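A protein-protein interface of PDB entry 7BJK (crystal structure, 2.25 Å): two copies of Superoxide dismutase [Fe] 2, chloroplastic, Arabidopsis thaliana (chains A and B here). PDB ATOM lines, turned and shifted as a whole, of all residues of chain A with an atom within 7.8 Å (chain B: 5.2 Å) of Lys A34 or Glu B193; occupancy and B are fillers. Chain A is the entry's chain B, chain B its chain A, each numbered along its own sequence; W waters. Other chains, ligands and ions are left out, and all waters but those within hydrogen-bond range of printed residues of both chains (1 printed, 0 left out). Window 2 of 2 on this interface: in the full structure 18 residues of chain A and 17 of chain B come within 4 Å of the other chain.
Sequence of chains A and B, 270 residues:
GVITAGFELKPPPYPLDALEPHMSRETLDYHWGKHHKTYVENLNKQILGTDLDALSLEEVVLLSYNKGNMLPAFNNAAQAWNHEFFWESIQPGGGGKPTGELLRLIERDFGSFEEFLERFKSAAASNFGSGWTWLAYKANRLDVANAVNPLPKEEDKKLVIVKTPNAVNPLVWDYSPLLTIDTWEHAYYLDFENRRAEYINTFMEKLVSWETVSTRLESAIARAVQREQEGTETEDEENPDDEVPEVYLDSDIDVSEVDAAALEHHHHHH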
ATOM      1  N   LEU A   9      11.225  10.655  -1.609  1.00  0.00           N
ATOM      2  CA  LEU A   9      11.412  12.059  -1.959  1.00  0.00           C
ATOM      3  C   LEU A   9      10.269  12.435  -2.892  1.00  0.00           C
ATOM      4  O   LEU A   9      10.267  12.078  -4.075  1.00  0.00           O
ATOM      5  CB  LEU A   9      12.767  12.289  -2.610  1.00  0.00           C
ATOM      6  CG  LEU A   9      13.001  13.733  -3.061  1.00  0.00           C
ATOM      7  CD1 LEU A   9      12.981  14.684  -1.872  1.00  0.00           C
ATOM      8  CD2 LEU A   9      14.307  13.854  -3.827  1.00  0.00           C
ATOM      9  N   THR A  27      17.800  26.750  -8.251  1.00  0.00           N
ATOM     10  CA  THR A  27      17.448  26.655  -6.840  1.00  0.00           C
ATOM     11  C   THR A  27      16.740  25.336  -6.550  1.00  0.00           C
ATOM     12  O   THR A  27      17.138  24.592  -5.648  1.00  0.00           O
ATOM     13  CB  THR A  27      16.591  27.860  -6.432  1.00  0.00           C
ATOM     14  OG1 THR A  27      17.354  29.055  -6.626  1.00  0.00           O
ATOM     15  CG2 THR A  27      16.210  27.777  -4.978  1.00  0.00           C
ATOM     16  N   LEU A  28      15.710  25.008  -7.332  1.00  0.00           N
ATOM     17  CA  LEU A  28      15.023  23.733  -7.137  1.00  0.00           C
ATOM     18  C   LEU A  28      15.990  22.558  -7.286  1.00  0.00           C
ATOM     19  O   LEU A  28      15.995  21.642  -6.453  1.00  0.00           O
ATOM     20  CB  LEU A  28      13.843  23.605  -8.113  1.00  0.00           C
ATOM     21  CG  LEU A  28      12.521  24.324  -7.771  1.00  0.00           C
ATOM     22  CD1 LEU A  28      11.746  23.590  -6.709  1.00  0.00           C
ATOM     23  CD2 LEU A  28      12.744  25.764  -7.329  1.00  0.00           C
ATOM     24  N   ASP A  29      16.829  22.571  -8.327  1.00  0.00           N
ATOM     25  CA  ASP A  29      17.779  21.475  -8.503  1.00  0.00           C
ATOM     26  C   ASP A  29      18.656  21.310  -7.278  1.00  0.00           C
ATOM     27  O   ASP A  29      18.904  20.181  -6.828  1.00  0.00           O
ATOM     28  CB  ASP A  29      18.648  21.695  -9.738  1.00  0.00           C
ATOM     29  CG  ASP A  29      17.899  21.432 -11.024  1.00  0.00           C
ATOM     30  OD1 ASP A  29      16.741  20.980 -10.936  1.00  0.00           O
ATOM     31  OD2 ASP A  29      18.461  21.675 -12.115  1.00  0.00           O
ATOM     32  N   TYR A  30      19.113  22.429  -6.703  1.00  0.00           N
ATOM     33  CA  TYR A  30      19.988  22.338  -5.544  1.00  0.00           C
ATOM     34  C   TYR A  30      19.198  22.054  -4.276  1.00  0.00           C
ATOM     35  O   TYR A  30      19.537  21.141  -3.513  1.00  0.00           O
ATOM     36  CB  TYR A  30      20.803  23.620  -5.395  1.00  0.00           C
ATOM     37  CG  TYR A  30      21.658  23.605  -4.155  1.00  0.00           C
ATOM     38  CD1 TYR A  30      22.586  22.576  -3.944  1.00  0.00           C
ATOM     39  CD2 TYR A  30      21.535  24.594  -3.187  1.00  0.00           C
ATOM     40  CE1 TYR A  30      23.373  22.534  -2.813  1.00  0.00           C
ATOM     41  CE2 TYR A  30      22.331  24.572  -2.039  1.00  0.00           C
ATOM     42  CZ  TYR A  30      23.250  23.538  -1.855  1.00  0.00           C
ATOM     43  OH  TYR A  30      24.041  23.499  -0.717  1.00  0.00           O
ATOM     44  N   HIS A  31      18.131  22.818  -4.047  1.00  0.00           N
ATOM     45  CA  HIS A  31      17.418  22.767  -2.775  1.00  0.00           C
ATOM     46  C   HIS A  31      16.575  21.501  -2.667  1.00  0.00           C
ATOM     47  O   HIS A  31      16.604  20.809  -1.645  1.00  0.00           O
ATOM     48  CB  HIS A  31      16.546  24.017  -2.626  1.00  0.00           C
ATOM     49  CG  HIS A  31      15.980  24.205  -1.254  1.00  0.00           C
ATOM     50  ND1 HIS A  31      15.106  25.226  -0.947  1.00  0.00           N
ATOM     51  CD2 HIS A  31      16.162  23.506  -0.107  1.00  0.00           C
ATOM     52  CE1 HIS A  31      14.783  25.158   0.334  1.00  0.00           C
ATOM     53  NE2 HIS A  31      15.414  24.126   0.868  1.00  0.00           N
ATOM     54  N   TRP A  32      15.795  21.196  -3.697  1.00  0.00           N
ATOM     55  CA  TRP A  32      15.080  19.927  -3.694  1.00  0.00           C
ATOM     56  C   TRP A  32      16.021  18.774  -4.027  1.00  0.00           C
ATOM     57  O   TRP A  32      16.125  17.814  -3.260  1.00  0.00           O
ATOM     58  CB  TRP A  32      13.907  19.971  -4.673  1.00  0.00           C
ATOM     59  CG  TRP A  32      13.170  18.661  -4.783  1.00  0.00           C
ATOM     60  CD1 TRP A  32      12.278  18.148  -3.887  1.00  0.00           C
ATOM     61  CD2 TRP A  32      13.281  17.701  -5.834  1.00  0.00           C
ATOM     62  NE1 TRP A  32      11.826  16.937  -4.316  1.00  0.00           N
ATOM     63  CE2 TRP A  32      12.416  16.634  -5.512  1.00  0.00           C
ATOM     64  CE3 TRP A  32      14.021  17.640  -7.014  1.00  0.00           C
ATOM     65  CZ2 TRP A  32      12.271  15.505  -6.329  1.00  0.00           C
ATOM     66  CZ3 TRP A  32      13.874  16.524  -7.833  1.00  0.00           C
ATOM     67  CH2 TRP A  32      13.005  15.466  -7.482  1.00  0.00           C
ATOM     68  N   GLY A  33      16.759  18.883  -5.136  1.00  0.00           N
ATOM     69  CA  GLY A  33      17.493  17.746  -5.665  1.00  0.00           C
ATOM     70  C   GLY A  33      18.687  17.314  -4.838  1.00  0.00           C
ATOM     71  O   GLY A  33      19.121  16.164  -4.949  1.00  0.00           O
ATOM     72  N   LYS A  34      19.243  18.203  -4.018  1.00  0.00           N
ATOM     73  CA  LYS A  34      20.359  17.817  -3.163  1.00  0.00           C
ATOM     74  C   LYS A  34      19.989  17.896  -1.688  1.00  0.00           C
ATOM     75  O   LYS A  34      20.072  16.879  -0.993  1.00  0.00           O
ATOM     76  CB  LYS A  34      21.595  18.674  -3.476  1.00  0.00           C
ATOM     77  CG  LYS A  34      22.128  18.438  -4.871  1.00  0.00           C
ATOM     78  CD  LYS A  34      23.598  18.792  -4.986  1.00  0.00           C
ATOM     79  CE  LYS A  34      24.130  18.454  -6.371  1.00  0.00           C
ATOM     80  NZ  LYS A  34      25.608  18.607  -6.455  1.00  0.00           N
ATOM     81  N   HIS A  35      19.551  19.058  -1.190  1.00  0.00           N
ATOM     82  CA  HIS A  35      19.306  19.187   0.245  1.00  0.00           C
ATOM     83  C   HIS A  35      18.132  18.324   0.697  1.00  0.00           C
ATOM     84  O   HIS A  35      18.258  17.538   1.645  1.00  0.00           O
ATOM     85  CB  HIS A  35      19.087  20.648   0.625  1.00  0.00           C
ATOM     86  CG  HIS A  35      20.358  21.360   0.955  1.00  0.00           C
ATOM     87  ND1 HIS A  35      21.028  21.169   2.147  1.00  0.00           N
ATOM     88  CD2 HIS A  35      21.107  22.229   0.236  1.00  0.00           C
ATOM     89  CE1 HIS A  35      22.130  21.898   2.149  1.00  0.00           C
ATOM     90  NE2 HIS A  35      22.194  22.561   1.008  1.00  0.00           N
ATOM     91  N   HIS A  36      16.968  18.492   0.059  1.00  0.00           N
ATOM     92  CA  HIS A  36      15.807  17.694   0.424  1.00  0.00           C
ATOM     93  C   HIS A  36      16.086  16.212   0.196  1.00  0.00           C
ATOM     94  O   HIS A  36      15.798  15.380   1.058  1.00  0.00           O
ATOM     95  CB  HIS A  36      14.583  18.142  -0.376  1.00  0.00           C
ATOM     96  CG  HIS A  36      13.292  17.560   0.115  1.00  0.00           C
ATOM     97  ND1 HIS A  36      12.071  17.889  -0.433  1.00  0.00           N
ATOM     98  CD2 HIS A  36      13.034  16.661   1.097  1.00  0.00           C
ATOM     99  CE1 HIS A  36      11.115  17.225   0.193  1.00  0.00           C
ATOM    100  NE2 HIS A  36      11.672  16.477   1.128  1.00  0.00           N
ATOM    101  N   LYS A  37      16.688  15.874  -0.946  1.00  0.00           N
ATOM    102  CA  LYS A  37      17.063  14.494  -1.208  1.00  0.00           C
ATOM    103  C   LYS A  37      17.962  13.955  -0.098  1.00  0.00           C
ATOM    104  O   LYS A  37      17.762  12.835   0.385  1.00  0.00           O
ATOM    105  CB  LYS A  37      17.754  14.402  -2.570  1.00  0.00           C
ATOM    106  CG  LYS A  37      18.078  12.984  -3.030  1.00  0.00           C
ATOM    107  CD  LYS A  37      19.116  12.980  -4.156  1.00  0.00           C
ATOM    108  CE  LYS A  37      20.489  13.447  -3.646  1.00  0.00           C
ATOM    109  NZ  LYS A  37      21.328  14.157  -4.677  1.00  0.00           N
ATOM    110  N   THR A  38      18.933  14.753   0.345  1.00  0.00           N
ATOM    111  CA  THR A  38      19.878  14.274   1.350  1.00  0.00           C
ATOM    112  C   THR A  38      19.194  14.033   2.692  1.00  0.00           C
ATOM    113  O   THR A  38      19.501  13.053   3.382  1.00  0.00           O
ATOM    114  CB  THR A  38      21.032  15.272   1.481  1.00  0.00           C
ATOM    115  OG1 THR A  38      21.815  15.226   0.279  1.00  0.00           O
ATOM    116  CG2 THR A  38      21.931  14.959   2.687  1.00  0.00           C
ATOM    117  N   TYR A  39      18.248  14.898   3.073  1.00  0.00           N
ATOM    118  CA  TYR A  39      17.506  14.682   4.315  1.00  0.00           C
ATOM    119  C   TYR A  39      16.791  13.333   4.303  1.00  0.00           C
ATOM    120  O   TYR A  39      16.876  12.564   5.269  1.00  0.00           O
ATOM    121  CB  TYR A  39      16.504  15.818   4.534  1.00  0.00           C
ATOM    122  CG  TYR A  39      17.142  17.155   4.917  1.00  0.00           C
ATOM    123  CD1 TYR A  39      18.057  17.239   5.964  1.00  0.00           C
ATOM    124  CD2 TYR A  39      16.824  18.322   4.242  1.00  0.00           C
ATOM    125  CE1 TYR A  39      18.631  18.446   6.324  1.00  0.00           C
ATOM    126  CE2 TYR A  39      17.405  19.567   4.606  1.00  0.00           C
ATOM    127  CZ  TYR A  39      18.307  19.608   5.639  1.00  0.00           C
ATOM    128  OH  TYR A  39      18.892  20.807   6.005  1.00  0.00           O
ATOM    129  N   VAL A  40      16.093  13.025   3.205  1.00  0.00           N
ATOM    130  CA  VAL A  40      15.345  11.778   3.107  1.00  0.00           C
ATOM    131  C   VAL A  40      16.296  10.589   3.079  1.00  0.00           C
ATOM    132  O   VAL A  40      16.114   9.617   3.821  1.00  0.00           O
ATOM    133  CB  VAL A  40      14.421  11.821   1.878  1.00  0.00           C
ATOM    134  CG1 VAL A  40      13.775  10.457   1.614  1.00  0.00           C
ATOM    135  CG2 VAL A  40      13.363  12.916   2.068  1.00  0.00           C
ATOM    136  N   GLU A  41      17.350  10.662   2.257  1.00  0.00           N
ATOM    137  CA  GLU A  41      18.346   9.593   2.250  1.00  0.00           C
ATOM    138  C   GLU A  41      18.948   9.381   3.637  1.00  0.00           C
ATOM    139  O   GLU A  41      19.056   8.240   4.101  1.00  0.00           O
ATOM    140  CB  GLU A  41      19.442   9.883   1.230  1.00  0.00           C
ATOM    141  CG  GLU A  41      19.010   9.664  -0.212  1.00  0.00           C
ATOM    142  CD  GLU A  41      20.120   9.949  -1.226  1.00  0.00           C
ATOM    143  OE1 GLU A  41      21.180  10.497  -0.828  1.00  0.00           O
ATOM    144  OE2 GLU A  41      19.924   9.625  -2.422  1.00  0.00           O
ATOM    145  N   HIS A 186      20.471  28.055   2.243  1.00  0.00           N
ATOM    146  CA  HIS A 186      20.393  27.329   0.979  1.00  0.00           C
ATOM    147  C   HIS A 186      19.070  27.584   0.267  1.00  0.00           C
ATOM    148  O   HIS A 186      18.970  27.365  -0.943  1.00  0.00           O
ATOM    149  CB  HIS A 186      20.630  25.816   1.202  1.00  0.00           C
ATOM    150  CG  HIS A 186      19.517  25.105   1.926  1.00  0.00           C
ATOM    151  ND1 HIS A 186      19.728  24.359   3.069  1.00  0.00           N
ATOM    152  CD2 HIS A 186      18.189  25.002   1.652  1.00  0.00           C
ATOM    153  CE1 HIS A 186      18.575  23.850   3.481  1.00  0.00           C
ATOM    154  NE2 HIS A 186      17.629  24.214   2.632  1.00  0.00           N
ATOM    155  N   LEU A 190      20.929  31.139  -4.269  1.00  0.00           N
ATOM    156  CA  LEU A 190      21.036  31.139  -5.729  1.00  0.00           C
ATOM    157  C   LEU A 190      20.156  32.199  -6.402  1.00  0.00           C
ATOM    158  O   LEU A 190      20.420  32.559  -7.557  1.00  0.00           O
ATOM    159  CB  LEU A 190      20.704  29.743  -6.263  1.00  0.00           C
ATOM    160  CG  LEU A 190      21.808  28.706  -6.022  1.00  0.00           C
ATOM    161  CD1 LEU A 190      21.296  27.297  -6.212  1.00  0.00           C
ATOM    162  CD2 LEU A 190      22.973  28.983  -6.965  1.00  0.00           C
ATOM    163  N   TYR B 188      30.714  27.609   2.709  1.00  0.00           N
ATOM    164  CA  TYR B 188      31.252  26.599   1.809  1.00  0.00           C
ATOM    165  C   TYR B 188      30.382  26.254   0.601  1.00  0.00           C
ATOM    166  O   TYR B 188      30.808  25.413  -0.206  1.00  0.00           O
ATOM    167  CB  TYR B 188      31.575  25.312   2.582  1.00  0.00           C
ATOM    168  CG  TYR B 188      30.408  24.702   3.331  1.00  0.00           C
ATOM    169  CD1 TYR B 188      30.083  25.124   4.606  1.00  0.00           C
ATOM    170  CD2 TYR B 188      29.642  23.687   2.769  1.00  0.00           C
ATOM    171  CE1 TYR B 188      29.017  24.565   5.305  1.00  0.00           C
ATOM    172  CE2 TYR B 188      28.585  23.121   3.466  1.00  0.00           C
ATOM    173  CZ  TYR B 188      28.277  23.566   4.734  1.00  0.00           C
ATOM    174  OH  TYR B 188      27.216  23.023   5.438  1.00  0.00           O
ATOM    175  N   TYR B 189      29.215  26.884   0.412  1.00  0.00           N
ATOM    176  CA  TYR B 189      28.413  26.553  -0.772  1.00  0.00           C
ATOM    177  C   TYR B 189      29.206  26.725  -2.065  1.00  0.00           C
ATOM    178  O   TYR B 189      29.204  25.842  -2.931  1.00  0.00           O
ATOM    179  CB  TYR B 189      27.143  27.400  -0.862  1.00  0.00           C
ATOM    180  CG  TYR B 189      26.535  27.162  -2.207  1.00  0.00           C
ATOM    181  CD1 TYR B 189      25.929  25.952  -2.489  1.00  0.00           C
ATOM    182  CD2 TYR B 189      26.650  28.098  -3.229  1.00  0.00           C
ATOM    183  CE1 TYR B 189      25.417  25.678  -3.744  1.00  0.00           C
ATOM    184  CE2 TYR B 189      26.141  27.843  -4.487  1.00  0.00           C
ATOM    185  CZ  TYR B 189      25.523  26.625  -4.743  1.00  0.00           C
ATOM    186  OH  TYR B 189      25.005  26.362  -5.995  1.00  0.00           O
ATOM    187  N   LEU B 190      29.880  27.871  -2.223  1.00  0.00           N
ATOM    188  CA  LEU B 190      30.498  28.195  -3.507  1.00  0.00           C
ATOM    189  C   LEU B 190      31.625  27.232  -3.874  1.00  0.00           C
ATOM    190  O   LEU B 190      31.925  27.055  -5.060  1.00  0.00           O
ATOM    191  CB  LEU B 190      31.009  29.637  -3.488  1.00  0.00           C
ATOM    192  CG  LEU B 190      29.900  30.653  -3.721  1.00  0.00           C
ATOM    193  CD1 LEU B 190      30.398  32.095  -3.571  1.00  0.00           C
ATOM    194  CD2 LEU B 190      29.318  30.420  -5.125  1.00  0.00           C
ATOM    195  N   ASP B 191      32.265  26.612  -2.884  1.00  0.00           N
ATOM    196  CA  ASP B 191      33.350  25.674  -3.136  1.00  0.00           C
ATOM    197  C   ASP B 191      32.931  24.219  -3.000  1.00  0.00           C
ATOM    198  O   ASP B 191      33.453  23.363  -3.714  1.00  0.00           O
ATOM    199  CB  ASP B 191      34.512  25.941  -2.177  1.00  0.00           C
ATOM    200  CG  ASP B 191      35.179  27.284  -2.419  1.00  0.00           C
ATOM    201  OD1 ASP B 191      35.520  27.585  -3.581  1.00  0.00           O
ATOM    202  OD2 ASP B 191      35.381  28.027  -1.443  1.00  0.00           O
ATOM    203  N   PHE B 192      32.000  23.910  -2.111  1.00  0.00           N
ATOM    204  CA  PHE B 192      31.674  22.527  -1.827  1.00  0.00           C
ATOM    205  C   PHE B 192      30.185  22.242  -1.905  1.00  0.00           C
ATOM    206  O   PHE B 192      29.775  21.105  -1.615  1.00  0.00           O
ATOM    207  CB  PHE B 192      32.211  22.135  -0.444  1.00  0.00           C
ATOM    208  CG  PHE B 192      33.699  22.210  -0.350  1.00  0.00           C
ATOM    209  CD1 PHE B 192      34.492  21.158  -0.805  1.00  0.00           C
ATOM    210  CD2 PHE B 192      34.317  23.349   0.147  1.00  0.00           C
ATOM    211  CE1 PHE B 192      35.872  21.227  -0.732  1.00  0.00           C
ATOM    212  CE2 PHE B 192      35.694  23.424   0.228  1.00  0.00           C
ATOM    213  CZ  PHE B 192      36.476  22.374  -0.216  1.00  0.00           C
ATOM    214  N   GLU B 193      29.377  23.226  -2.322  1.00  0.00           N
ATOM    215  CA  GLU B 193      27.925  23.114  -2.307  1.00  0.00           C
ATOM    216  C   GLU B 193      27.482  22.673  -0.923  1.00  0.00           C
ATOM    217  O   GLU B 193      27.789  23.354   0.064  1.00  0.00           O
ATOM    218  CB  GLU B 193      27.431  22.157  -3.389  1.00  0.00           C
ATOM    219  CG  GLU B 193      27.692  22.672  -4.789  1.00  0.00           C
ATOM    220  CD  GLU B 193      27.294  21.662  -5.855  1.00  0.00           C
ATOM    221  OE1 GLU B 193      28.124  20.784  -6.182  1.00  0.00           O
ATOM    222  OE2 GLU B 193      26.144  21.737  -6.354  1.00  0.00           O
ATOM    223  N   ASN B 194      26.804  21.525  -0.831  1.00  0.00           N
ATOM    224  CA  ASN B 194      26.296  21.057   0.449  1.00  0.00           C
ATOM    225  C   ASN B 194      27.230  20.064   1.130  1.00  0.00           C
ATOM    226  O   ASN B 194      26.913  19.590   2.222  1.00  0.00           O
ATOM    227  CB  ASN B 194      24.896  20.450   0.276  1.00  0.00           C
ATOM    228  CG  ASN B 194      24.901  19.186  -0.558  1.00  0.00           C
ATOM    229  OD1 ASN B 194      25.486  19.138  -1.642  1.00  0.00           O
ATOM    230  ND2 ASN B 194      24.238  18.148  -0.056  1.00  0.00           N
ATOM    231  N   ARG B 195      28.396  19.780   0.547  1.00  0.00           N
ATOM    232  CA  ARG B 195      29.287  18.735   1.063  1.00  0.00           C
ATOM    233  C   ARG B 195      30.226  19.300   2.137  1.00  0.00           C
ATOM    234  O   ARG B 195      31.437  19.473   1.946  1.00  0.00           O
ATOM    235  CB  ARG B 195      30.044  18.098  -0.092  1.00  0.00           C
ATOM    236  CG  ARG B 195      29.123  17.703  -1.238  1.00  0.00           C
ATOM    237  CD  ARG B 195      29.908  17.062  -2.362  1.00  0.00           C
ATOM    238  NE  ARG B 195      30.892  17.997  -2.889  1.00  0.00           N
ATOM    239  CZ  ARG B 195      30.617  18.895  -3.822  1.00  0.00           C
ATOM    240  NH1 ARG B 195      29.390  18.969  -4.322  1.00  0.00           N
ATOM    241  NH2 ARG B 195      31.563  19.720  -4.246  1.00  0.00           N
HETATM  242  O   HOH W   1      26.924  17.813  -3.623  1.00  0.00           O
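Among the printed residues, merely in contact across the chains: Tyr A30 with Tyr B189, Tyr A30 with Glu B193, Lys A34 with Asn B194, His A35 with Asn B194, Thr A38 with Asn B194 and Leu A190 with Tyr B189.
Of the 18 printed residues of chain A, 5 touch a printed residue of chain B. Hydrophobic or aromatic side chains of chain A within 4 Å of the printed part of chain B: Tyr A30, His A35 and Leu A190. Of the 8 printed residues of chain B, 3 touch a printed residue of chain A. Hydrophobic or aromatic side chains of chain B that line the printed part of chain A: Tyr B189. Among the printed residues, Asp or Glu carboxylates within 4 Å of a Lys or Arg side-chain nitrogen of the other chain: Lys A34 with Glu B193 (3.2 Å).
Position printed for both chains: 190. Of the 8 pairs that touch across the chains among the printed residues, none has its exchanged pair printed and touching as well.
The side-chain amino group of Lys A34 is in salt-bridge range of the side-chain carboxylate of Glu B193 (3.2 Å). The side-chain hydroxyl of Tyr A30 lies close to the backbone NH of Asn B194 (3.4 Å).
Printed residues of chain B within 4 Å of Tyr A30: Tyr B189 (3.6 Å), Glu B193 (3.5 Å) and Asn B194 (3.3 Å). Lys A34 touches just these residues of chain B: Glu B193 and Asn B194. Of the printed residues of chain A, Tyr B189 touches Tyr A30 and Leu A190. Of chain A, only Tyr A30 (3.5 Å) and Lys A34 (3.2 Å) come within 4 Å of Glu B193. The nearest residue of chain A that does not touch Glu B193 is His A35 (5.6 Å). The nearest printed residue of chain B that does not touch Leu A190 is Leu B190 (6.8 Å).
Water W1 lies within hydrogen-bond range of the side-chain amide oxygen of Asn B194, the guanidinium group of Arg B195 and the side-chain amino group of Lys A34.
The backbone carbonyl oxygen (O) of Asp A29 lies within hydrogen-bond range of the backbone NH (N) of Lys A34 (3.5 Å). O of Tyr B188 lies within hydrogen-bond range of N of Glu B193, 3.4 Å away. OH of Tyr A30 is in hydrogen-bond range of NE2 of His A35, 2.7 Å away. O of Lys A34 is in hydrogen-bond range of OG1 of Thr A38. The side-chain carboxylate (OE1) of Glu B193 is in salt-bridge range of the guanidinium group (NH1) of Arg B195, 2.9 Å away.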
